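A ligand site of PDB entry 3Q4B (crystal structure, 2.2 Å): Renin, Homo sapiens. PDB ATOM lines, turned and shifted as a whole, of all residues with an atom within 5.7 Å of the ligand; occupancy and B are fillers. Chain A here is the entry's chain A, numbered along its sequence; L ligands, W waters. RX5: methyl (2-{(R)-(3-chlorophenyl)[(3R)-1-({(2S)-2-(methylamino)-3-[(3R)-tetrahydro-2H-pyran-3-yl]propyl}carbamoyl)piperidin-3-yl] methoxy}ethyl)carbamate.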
ATOM      1  N   THR A  18      -0.518   5.348   7.547  1.00  0.00           N
ATOM      2  CA  THR A  18      -1.032   5.515   8.913  1.00  0.00           C
ATOM      3  C   THR A  18      -0.173   6.373   9.808  1.00  0.00           C
ATOM      4  O   THR A  18      -0.662   6.879  10.817  1.00  0.00           O
ATOM      5  CB  THR A  18      -1.154   4.172   9.616  1.00  0.00           C
ATOM      6  OG1 THR A  18       0.120   3.521   9.549  1.00  0.00           O
ATOM      7  CG2 THR A  18      -2.272   3.333   8.934  1.00  0.00           C
ATOM      8  N   GLN A  19       1.104   6.535   9.488  1.00  0.00           N
ATOM      9  CA  GLN A  19       1.925   7.447  10.273  1.00  0.00           C
ATOM     10  C   GLN A  19       2.712   8.346   9.372  1.00  0.00           C
ATOM     11  O   GLN A  19       3.469   7.850   8.534  1.00  0.00           O
ATOM     12  CB  GLN A  19       2.896   6.680  11.239  1.00  0.00           C
ATOM     13  CG  GLN A  19       2.155   5.758  12.234  1.00  0.00           C
ATOM     14  CD  GLN A  19       3.118   4.996  13.112  1.00  0.00           C
ATOM     15  OE1 GLN A  19       4.180   5.497  13.445  1.00  0.00           O
ATOM     16  NE2 GLN A  19       2.754   3.780  13.492  1.00  0.00           N
ATOM     17  N   TYR A  20       2.554   9.664   9.548  1.00  0.00           N
ATOM     18  CA  TYR A  20       3.295  10.664   8.793  1.00  0.00           C
ATOM     19  C   TYR A  20       4.010  11.556   9.792  1.00  0.00           C
ATOM     20  O   TYR A  20       3.428  12.015  10.786  1.00  0.00           O
ATOM     21  CB  TYR A  20       2.360  11.574   7.939  1.00  0.00           C
ATOM     22  CG  TYR A  20       1.553  10.907   6.818  1.00  0.00           C
ATOM     23  CD1 TYR A  20       0.383  10.216   7.125  1.00  0.00           C
ATOM     24  CD2 TYR A  20       1.930  10.997   5.494  1.00  0.00           C
ATOM     25  CE1 TYR A  20      -0.364   9.595   6.119  1.00  0.00           C
ATOM     26  CE2 TYR A  20       1.203  10.409   4.452  1.00  0.00           C
ATOM     27  CZ  TYR A  20       0.037   9.677   4.768  1.00  0.00           C
ATOM     28  OH  TYR A  20      -0.773   9.090   3.788  1.00  0.00           O
ATOM     29  N   TYR A  21       5.281  11.807   9.518  1.00  0.00           N
ATOM     30  CA  TYR A  21       6.131  12.430  10.536  1.00  0.00           C
ATOM     31  C   TYR A  21       7.344  13.025   9.859  1.00  0.00           C
ATOM     32  O   TYR A  21       7.697  12.624   8.776  1.00  0.00           O
ATOM     33  CB  TYR A  21       6.494  11.422  11.655  1.00  0.00           C
ATOM     34  CG  TYR A  21       7.335  10.248  11.174  1.00  0.00           C
ATOM     35  CD1 TYR A  21       8.729  10.394  10.935  1.00  0.00           C
ATOM     36  CD2 TYR A  21       6.742   9.002  10.943  1.00  0.00           C
ATOM     37  CE1 TYR A  21       9.483   9.321  10.500  1.00  0.00           C
ATOM     38  CE2 TYR A  21       7.466   7.935  10.502  1.00  0.00           C
ATOM     39  CZ  TYR A  21       8.846   8.097  10.275  1.00  0.00           C
ATOM     40  OH  TYR A  21       9.556   7.011   9.826  1.00  0.00           O
ATOM     41  N   VAL A  36       5.285  13.773  14.836  1.00  0.00           N
ATOM     42  CA  VAL A  36       4.019  13.971  14.135  1.00  0.00           C
ATOM     43  C   VAL A  36       3.539  15.389  14.370  1.00  0.00           C
ATOM     44  O   VAL A  36       3.465  15.811  15.486  1.00  0.00           O
ATOM     45  CB  VAL A  36       2.963  12.915  14.585  1.00  0.00           C
ATOM     46  CG1 VAL A  36       1.581  13.236  13.975  1.00  0.00           C
ATOM     47  CG2 VAL A  36       3.415  11.535  14.170  1.00  0.00           C
ATOM     48  N   ASP A  38       0.515  17.563  14.636  1.00  0.00           N
ATOM     49  CA  ASP A  38      -0.819  17.152  15.047  1.00  0.00           C
ATOM     50  C   ASP A  38      -1.725  18.360  15.219  1.00  0.00           C
ATOM     51  O   ASP A  38      -1.575  19.106  16.210  1.00  0.00           O
ATOM     52  CB  ASP A  38      -0.767  16.342  16.373  1.00  0.00           C
ATOM     53  CG  ASP A  38      -2.123  15.777  16.789  1.00  0.00           C
ATOM     54  OD1 ASP A  38      -3.067  15.738  15.966  1.00  0.00           O
ATOM     55  OD2 ASP A  38      -2.287  15.400  17.961  1.00  0.00           O
ATOM     56  N   GLY A  40      -4.763  18.199  16.093  1.00  0.00           N
ATOM     57  CA  GLY A  40      -5.728  17.887  17.167  1.00  0.00           C
ATOM     58  C   GLY A  40      -5.107  18.002  18.521  1.00  0.00           C
ATOM     59  O   GLY A  40      -5.721  17.635  19.516  1.00  0.00           O
ATOM     60  N   SER A  41      -3.882  18.520  18.601  1.00  0.00           N
ATOM     61  CA  SER A  41      -3.301  18.764  19.915  1.00  0.00           C
ATOM     62  C   SER A  41      -2.383  19.978  19.852  1.00  0.00           C
ATOM     63  O   SER A  41      -2.194  20.543  18.753  1.00  0.00           O
ATOM     64  CB  SER A  41      -2.602  17.516  20.505  1.00  0.00           C
ATOM     65  OG  SER A  41      -1.425  17.163  19.782  1.00  0.00           O
ATOM     66  N   TRP A  45       6.224  17.579  22.508  1.00  0.00           N
ATOM     67  CA  TRP A  45       6.990  16.653  23.417  1.00  0.00           C
ATOM     68  C   TRP A  45       7.882  15.661  22.664  1.00  0.00           C
ATOM     69  O   TRP A  45       7.589  15.275  21.560  1.00  0.00           O
ATOM     70  CB  TRP A  45       6.140  15.938  24.459  1.00  0.00           C
ATOM     71  CG  TRP A  45       5.202  14.921  23.856  1.00  0.00           C
ATOM     72  CD1 TRP A  45       3.928  15.146  23.484  1.00  0.00           C
ATOM     73  CD2 TRP A  45       5.477  13.543  23.542  1.00  0.00           C
ATOM     74  NE1 TRP A  45       3.366  14.018  22.955  1.00  0.00           N
ATOM     75  CE2 TRP A  45       4.291  13.007  22.980  1.00  0.00           C
ATOM     76  CE3 TRP A  45       6.592  12.704  23.701  1.00  0.00           C
ATOM     77  CZ2 TRP A  45       4.183  11.659  22.552  1.00  0.00           C
ATOM     78  CZ3 TRP A  45       6.492  11.318  23.258  1.00  0.00           C
ATOM     79  CH2 TRP A  45       5.284  10.836  22.683  1.00  0.00           C
ATOM     80  N   TYR A  83      -3.892  11.344  25.422  1.00  0.00           N
ATOM     81  CA  TYR A  83      -4.497  11.272  24.132  1.00  0.00           C
ATOM     82  C   TYR A  83      -5.470  10.091  24.102  1.00  0.00           C
ATOM     83  O   TYR A  83      -5.602   9.363  25.082  1.00  0.00           O
ATOM     84  CB  TYR A  83      -3.425  11.099  23.071  1.00  0.00           C
ATOM     85  CG  TYR A  83      -2.389  12.214  23.014  1.00  0.00           C
ATOM     86  CD1 TYR A  83      -2.655  13.379  22.352  1.00  0.00           C
ATOM     87  CD2 TYR A  83      -1.138  12.044  23.609  1.00  0.00           C
ATOM     88  CE1 TYR A  83      -1.683  14.382  22.251  1.00  0.00           C
ATOM     89  CE2 TYR A  83      -0.171  13.033  23.551  1.00  0.00           C
ATOM     90  CZ  TYR A  83      -0.435  14.192  22.860  1.00  0.00           C
ATOM     91  OH  TYR A  83       0.529  15.170  22.821  1.00  0.00           O
ATOM     92  N   SER A  84      -6.105   9.891  22.952  1.00  0.00           N
ATOM     93  CA  SER A  84      -6.861   8.698  22.639  1.00  0.00           C
ATOM     94  C   SER A  84      -5.978   7.463  22.808  1.00  0.00           C
ATOM     95  O   SER A  84      -6.415   6.432  23.308  1.00  0.00           O
ATOM     96  CB  SER A  84      -7.314   8.798  21.191  1.00  0.00           C
ATOM     97  OG  SER A  84      -6.167   8.860  20.337  1.00  0.00           O
ATOM     98  N   THR A  85      -4.711   7.560  22.401  1.00  0.00           N
ATOM     99  CA  THR A  85      -3.752   6.415  22.473  1.00  0.00           C
ATOM    100  C   THR A  85      -3.204   6.073  23.855  1.00  0.00           C
ATOM    101  O   THR A  85      -2.714   4.984  24.067  1.00  0.00           O
ATOM    102  CB  THR A  85      -2.465   6.688  21.612  1.00  0.00           C
ATOM    103  OG1 THR A  85      -1.858   7.930  22.005  1.00  0.00           O
ATOM    104  CG2 THR A  85      -2.732   6.694  20.158  1.00  0.00           C
ATOM    105  N   PRO A 118       0.441   2.612  23.148  1.00  0.00           N
ATOM    106  CA  PRO A 118       0.794   2.027  21.905  1.00  0.00           C
ATOM    107  C   PRO A 118       2.140   2.529  21.361  1.00  0.00           C
ATOM    108  O   PRO A 118       2.440   2.310  20.188  1.00  0.00           O
ATOM    109  CB  PRO A 118      -0.327   2.556  21.033  1.00  0.00           C
ATOM    110  CG  PRO A 118      -0.287   4.039  21.431  1.00  0.00           C
ATOM    111  CD  PRO A 118       0.013   4.003  22.935  1.00  0.00           C
ATOM    112  N   PHE A 119       2.961   3.181  22.192  1.00  0.00           N
ATOM    113  CA  PHE A 119       4.229   3.782  21.700  1.00  0.00           C
ATOM    114  C   PHE A 119       5.248   2.811  21.182  1.00  0.00           C
ATOM    115  O   PHE A 119       6.127   3.201  20.392  1.00  0.00           O
ATOM    116  CB  PHE A 119       4.827   4.801  22.667  1.00  0.00           C
ATOM    117  CG  PHE A 119       3.977   6.023  22.793  1.00  0.00           C
ATOM    118  CD1 PHE A 119       4.000   7.012  21.809  1.00  0.00           C
ATOM    119  CD2 PHE A 119       3.042   6.138  23.830  1.00  0.00           C
ATOM    120  CE1 PHE A 119       3.122   8.131  21.855  1.00  0.00           C
ATOM    121  CE2 PHE A 119       2.153   7.258  23.895  1.00  0.00           C
ATOM    122  CZ  PHE A 119       2.201   8.246  22.931  1.00  0.00           C
ATOM    123  N   LEU A 121       4.616   0.972  18.952  1.00  0.00           N
ATOM    124  CA  LEU A 121       4.215   0.865  17.537  1.00  0.00           C
ATOM    125  C   LEU A 121       4.412   2.192  16.840  1.00  0.00           C
ATOM    126  O   LEU A 121       4.115   2.272  15.655  1.00  0.00           O
ATOM    127  CB  LEU A 121       2.741   0.452  17.366  1.00  0.00           C
ATOM    128  CG  LEU A 121       2.211  -0.838  18.034  1.00  0.00           C
ATOM    129  CD1 LEU A 121       0.714  -0.853  18.114  1.00  0.00           C
ATOM    130  CD2 LEU A 121       2.744  -2.118  17.350  1.00  0.00           C
ATOM    131  N   ALA A 122       4.810   3.241  17.586  1.00  0.00           N
ATOM    132  CA  ALA A 122       5.060   4.516  16.914  1.00  0.00           C
ATOM    133  C   ALA A 122       6.374   4.432  16.203  1.00  0.00           C
ATOM    134  O   ALA A 122       7.426   4.113  16.822  1.00  0.00           O
ATOM    135  CB  ALA A 122       5.109   5.694  17.908  1.00  0.00           C
ATOM    136  N   PHE A 124       7.503   7.245  15.082  1.00  0.00           N
ATOM    137  CA  PHE A 124       7.965   8.576  15.428  1.00  0.00           C
ATOM    138  C   PHE A 124       8.452   8.637  16.897  1.00  0.00           C
ATOM    139  O   PHE A 124       8.125   7.777  17.734  1.00  0.00           O
ATOM    140  CB  PHE A 124       6.800   9.564  15.176  1.00  0.00           C
ATOM    141  CG  PHE A 124       5.490   9.161  15.846  1.00  0.00           C
ATOM    142  CD1 PHE A 124       4.638   8.255  15.248  1.00  0.00           C
ATOM    143  CD2 PHE A 124       5.136   9.711  17.069  1.00  0.00           C
ATOM    144  CE1 PHE A 124       3.426   7.896  15.880  1.00  0.00           C
ATOM    145  CE2 PHE A 124       3.988   9.371  17.707  1.00  0.00           C
ATOM    146  CZ  PHE A 124       3.096   8.454  17.128  1.00  0.00           C
ATOM    147  N   VAL A 127       5.588  14.463  19.333  1.00  0.00           N
ATOM    148  CA  VAL A 127       4.463  15.163  18.723  1.00  0.00           C
ATOM    149  C   VAL A 127       4.717  16.635  18.780  1.00  0.00           C
ATOM    150  O   VAL A 127       5.254  17.143  19.767  1.00  0.00           O
ATOM    151  CB  VAL A 127       3.174  14.850  19.476  1.00  0.00           C
ATOM    152  CG1 VAL A 127       1.990  15.653  18.908  1.00  0.00           C
ATOM    153  CG2 VAL A 127       2.916  13.359  19.392  1.00  0.00           C
ATOM    154  N   TYR A 162      -0.500  15.107   2.233  1.00  0.00           N
ATOM    155  CA  TYR A 162      -0.198  13.742   2.642  1.00  0.00           C
ATOM    156  C   TYR A 162      -0.325  12.829   1.420  1.00  0.00           C
ATOM    157  O   TYR A 162      -1.417  12.721   0.858  1.00  0.00           O
ATOM    158  CB  TYR A 162      -1.194  13.236   3.691  1.00  0.00           C
ATOM    159  CG  TYR A 162      -0.959  13.603   5.182  1.00  0.00           C
ATOM    160  CD1 TYR A 162       0.200  14.229   5.594  1.00  0.00           C
ATOM    161  CD2 TYR A 162      -1.914  13.231   6.160  1.00  0.00           C
ATOM    162  CE1 TYR A 162       0.419  14.521   6.918  1.00  0.00           C
ATOM    163  CE2 TYR A 162      -1.712  13.545   7.526  1.00  0.00           C
ATOM    164  CZ  TYR A 162      -0.547  14.185   7.894  1.00  0.00           C
ATOM    165  OH  TYR A 162      -0.300  14.488   9.219  1.00  0.00           O
ATOM    166  N   LEU A 224     -13.606  17.687  13.179  1.00  0.00           N
ATOM    167  CA  LEU A 224     -12.329  18.179  13.618  1.00  0.00           C
ATOM    168  C   LEU A 224     -11.414  17.794  12.467  1.00  0.00           C
ATOM    169  O   LEU A 224     -11.481  16.674  12.006  1.00  0.00           O
ATOM    170  CB  LEU A 224     -11.931  17.390  14.877  1.00  0.00           C
ATOM    171  CG  LEU A 224     -10.489  17.485  15.369  1.00  0.00           C
ATOM    172  CD1 LEU A 224     -10.292  18.895  15.847  1.00  0.00           C
ATOM    173  CD2 LEU A 224     -10.190  16.492  16.546  1.00  0.00           C
ATOM    174  N   ASP A 226      -8.029  16.692  11.692  1.00  0.00           N
ATOM    175  CA  ASP A 226      -6.996  16.177  12.601  1.00  0.00           C
ATOM    176  C   ASP A 226      -5.819  15.531  11.863  1.00  0.00           C
ATOM    177  O   ASP A 226      -5.909  14.366  11.498  1.00  0.00           O
ATOM    178  CB  ASP A 226      -7.578  15.117  13.569  1.00  0.00           C
ATOM    179  CG  ASP A 226      -6.608  14.827  14.710  1.00  0.00           C
ATOM    180  OD1 ASP A 226      -5.430  15.258  14.607  1.00  0.00           O
ATOM    181  OD2 ASP A 226      -7.018  14.215  15.681  1.00  0.00           O
ATOM    182  N   THR A 227      -4.739  16.258  11.715  1.00  0.00           N
ATOM    183  CA  THR A 227      -3.601  15.756  10.988  1.00  0.00           C
ATOM    184  C   THR A 227      -2.862  14.642  11.783  1.00  0.00           C
ATOM    185  O   THR A 227      -2.035  13.927  11.193  1.00  0.00           O
ATOM    186  CB  THR A 227      -2.629  16.890  10.588  1.00  0.00           C
ATOM    187  OG1 THR A 227      -2.135  17.544  11.763  1.00  0.00           O
ATOM    188  CG2 THR A 227      -3.298  17.911   9.654  1.00  0.00           C
ATOM    189  N   GLY A 228      -3.179  14.482  13.085  1.00  0.00           N
ATOM    190  CA  GLY A 228      -2.606  13.391  13.847  1.00  0.00           C
ATOM    191  C   GLY A 228      -3.451  12.102  13.799  1.00  0.00           C
ATOM    192  O   GLY A 228      -3.056  11.055  14.393  1.00  0.00           O
ATOM    193  N   ALA A 229      -4.600  12.165  13.125  1.00  0.00           N
ATOM    194  CA  ALA A 229      -5.484  11.006  12.996  1.00  0.00           C
ATOM    195  C   ALA A 229      -5.184  10.212  11.715  1.00  0.00           C
ATOM    196  O   ALA A 229      -5.147  10.809  10.586  1.00  0.00           O
ATOM    197  CB  ALA A 229      -7.005  11.399  13.015  1.00  0.00           C
ATOM    198  N   SER A 230      -5.008   8.898  11.847  1.00  0.00           N
ATOM    199  CA  SER A 230      -4.708   8.101  10.648  1.00  0.00           C
ATOM    200  C   SER A 230      -5.944   7.989   9.764  1.00  0.00           C
ATOM    201  O   SER A 230      -5.853   8.075   8.536  1.00  0.00           O
ATOM    202  CB  SER A 230      -4.196   6.687  10.996  1.00  0.00           C
ATOM    203  OG  SER A 230      -3.148   6.786  11.949  1.00  0.00           O
ATOM    204  N   HIS A 301     -12.811   4.337  11.415  1.00  0.00           N
ATOM    205  CA  HIS A 301     -13.121   3.640  12.663  1.00  0.00           C
ATOM    206  C   HIS A 301     -13.954   4.557  13.560  1.00  0.00           C
ATOM    207  O   HIS A 301     -14.145   5.745  13.247  1.00  0.00           O
ATOM    208  CB  HIS A 301     -11.846   3.170  13.410  1.00  0.00           C
ATOM    209  CG  HIS A 301     -10.947   4.285  13.887  1.00  0.00           C
ATOM    210  ND1 HIS A 301     -10.206   4.188  15.045  1.00  0.00           N
ATOM    211  CD2 HIS A 301     -10.667   5.509  13.362  1.00  0.00           C
ATOM    212  CE1 HIS A 301      -9.511   5.300  15.223  1.00  0.00           C
ATOM    213  NE2 HIS A 301      -9.779   6.120  14.221  1.00  0.00           N
ATOM    214  N   MET A 303     -14.539   6.554  17.118  1.00  0.00           N
ATOM    215  CA  MET A 303     -13.838   7.217  18.210  1.00  0.00           C
ATOM    216  C   MET A 303     -14.816   8.142  18.942  1.00  0.00           C
ATOM    217  O   MET A 303     -15.281   9.112  18.361  1.00  0.00           O
ATOM    218  CB  MET A 303     -12.689   8.056  17.693  1.00  0.00           C
ATOM    219  CG  MET A 303     -11.414   7.307  17.459  1.00  0.00           C
ATOM    220  SD  MET A 303     -10.201   7.648  18.763  1.00  0.00           S
ATOM    221  CE  MET A 303     -10.626   9.343  19.116  1.00  0.00           C
ATOM    222  N   GLY A 316      -9.109  12.603   9.253  1.00  0.00           N
ATOM    223  CA  GLY A 316      -7.700  12.368   9.363  1.00  0.00           C
ATOM    224  C   GLY A 316      -7.033  12.118   8.013  1.00  0.00           C
ATOM    225  O   GLY A 316      -7.491  12.634   6.982  1.00  0.00           O
ATOM    226  N   ALA A 317      -5.940  11.355   8.005  1.00  0.00           N
ATOM    227  CA  ALA A 317      -5.146  11.199   6.766  1.00  0.00           C
ATOM    228  C   ALA A 317      -5.930  10.576   5.590  1.00  0.00           C
ATOM    229  O   ALA A 317      -5.686  10.938   4.459  1.00  0.00           O
ATOM    230  CB  ALA A 317      -3.877  10.422   7.011  1.00  0.00           C
HETATM  231  C1  RX5 L   1      -5.378  14.383  18.537  1.00  0.00           C
HETATM  232  N1  RX5 L   1      -4.582  13.993  17.359  1.00  0.00           N
HETATM  233  O1  RX5 L   1      -6.515   9.377  17.612  1.00  0.00           O
HETATM  234  C2  RX5 L   1      -4.173  12.571  17.332  1.00  0.00           C
HETATM  235  N2  RX5 L   1      -4.867  10.348  16.557  1.00  0.00           N
HETATM  236  O2  RX5 L   1      -1.153   7.989  15.301  1.00  0.00           O
HETATM  237  C3  RX5 L   1      -5.343  11.611  17.151  1.00  0.00           C
HETATM  238  N3  RX5 L   1      -5.185   8.051  16.366  1.00  0.00           N
HETATM  239  O3  RX5 L   1       0.218  10.085  11.356  1.00  0.00           O
HETATM  240  C4  RX5 L   1      -5.546   9.251  16.846  1.00  0.00           C
HETATM  241  N4  RX5 L   1      -0.902  10.091  13.411  1.00  0.00           N
HETATM  242  O4  RX5 L   1      -1.939  10.913  11.452  1.00  0.00           O
HETATM  243  C5  RX5 L   1      -4.035   7.797  15.457  1.00  0.00           C
HETATM  244  C6  RX5 L   1      -3.028   6.948  16.265  1.00  0.00           C
HETATM  245  C7  RX5 L   1      -3.701   5.624  16.719  1.00  0.00           C
HETATM  246  C8  RX5 L   1      -5.038   5.848  17.451  1.00  0.00           C
HETATM  247  C9  RX5 L   1      -5.973   6.849  16.718  1.00  0.00           C
HETATM  248  C10 RX5 L   1      -1.728   6.701  15.477  1.00  0.00           C
HETATM  249  C11 RX5 L   1      -3.364  12.261  18.573  1.00  0.00           C
HETATM  250  C12 RX5 L   1      -2.320  11.157  18.415  1.00  0.00           C
HETATM  251  C13 RX5 L   1      -2.067  10.556  19.794  1.00  0.00           C
HETATM  252  O14 RX5 L   1      -1.074   9.510  19.699  1.00  0.00           O
HETATM  253  C15 RX5 L   1       0.199  10.084  19.390  1.00  0.00           C
HETATM  254  C16 RX5 L   1       0.131  10.762  18.031  1.00  0.00           C
HETATM  255  C17 RX5 L   1      -1.005  11.748  17.939  1.00  0.00           C
HETATM  256  C18 RX5 L   1      -0.139   7.972  14.271  1.00  0.00           C
HETATM  257  C19 RX5 L   1       0.244   9.430  14.072  1.00  0.00           C
HETATM  258  C20 RX5 L   1      -0.791  10.340  12.082  1.00  0.00           C
HETATM  259  C21 RX5 L   1      -0.715   5.875  16.205  1.00  0.00           C
HETATM  260  C22 RX5 L   1      -0.100   6.338  17.365  1.00  0.00           C
HETATM  261  C23 RX5 L   1       0.838   5.549  18.015  1.00  0.00           C
HETATM  262  C24 RX5 L   1       1.215   4.299  17.560  1.00  0.00           C
HETATM  263  C25 RX5 L   1       0.584   3.851  16.396  1.00  0.00           C
HETATM  264  C26 RX5 L   1      -0.375   4.609  15.741  1.00  0.00           C
HETATM  265  C27 RX5 L   1      -2.016  10.930  10.012  1.00  0.00           C
HETATM  266 CL2  RX5 L   1       1.571   6.170  19.510  1.00  0.00          CL
HETATM  267  O   HOH W   1      -8.254  11.360  19.057  1.00  0.00           O
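An oxygen (O14) of the ligand lies within hydrogen-bond range of the side-chain hydroxyl (OG1) of Thr 85 (2.9 Å).
The backbone NH of Ala 229 sits close to an oxygen (O4) of the ligand.
N1 of the ligand lies within salt-bridge range of OD2 of Asp 226, 3.0 Å away.
O of Gly 228 is in hydrogen-bond range of N4 of the ligand (2.6 Å).
OG of Ser 84 sits at hydrogen-bond distance from O1 of the ligand (2.8 Å).
An oxygen (O3) of the ligand is in hydrogen-bond range of the backbone NH of Tyr 20, 3.0 Å away.
The side-chain carboxylate (OD1) of Asp 38 is in salt-bridge range of a nitrogen (N1) of the ligand.
The backbone NH (N) of Gly 228 lies within hydrogen-bond range of the side-chain carboxylate (OD1) of Asp 226 (2.8 Å).
OD1 of Asp 226 sits at hydrogen-bond distance from N of Gly 40 (3.4 Å).
The backbone NH (N) of Gly 40 sits at hydrogen-bond distance from the side-chain carboxylate (OD1) of Asp 38, 3.0 Å away.
The backbone carbonyl oxygen (O) of Ala 229 is in hydrogen-bond range of the backbone NH (N) of Ala 317.
O of Thr 18 lies within hydrogen-bond range of OG of Ser 230 (2.7 Å).
The side-chain hydroxyl (OG) of Ser 41 is in hydrogen-bond range of the side-chain carboxylate (OD2) of Asp 38, 2.7 Å away.
The side-chain hydroxyl (OH) of Tyr 83 sits at hydrogen-bond distance from the indole nitrogen (NE1) of Trp 45 (3.1 Å).
The backbone carbonyl oxygen of Leu 121 is in hydrogen-bond range of the side-chain amide nitrogen of Gln 19, at 3.0 Å.
The backbone carbonyl oxygen of Thr 18 sits close to an oxygen (O3) of the ligand (3.4 Å).
The backbone carbonyl oxygen of Thr 227 lies close to an oxygen (O4) of the ligand (3.0 Å).
Residues that only touch the ligand: Gln 19 (3.3 Å), Gly 40 (3.4 Å), Pro 118 (3.4 Å), Phe 119 (3.4 Å), Ala 317 (3.6 Å), Tyr 83 (3.6 Å), Tyr 162 (3.6 Å), Phe 124 (3.6 Å), Ser 230 (3.7 Å), Ala 122 (3.7 Å), Val 36 (3.8 Å) and Leu 121 (3.9 Å).
Hydrophobic or aromatic side chains that line the ligand: Tyr 20, Val 36, Tyr 83, Pro 118, Phe 119, Ala 122, Phe 124, Tyr 162 and Ala 317.
Water W1 lies within hydrogen-bond range of an oxygen (O1) of the ligand (3.0 Å) and the side-chain hydroxyl of Ser 84 (3.5 Å).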
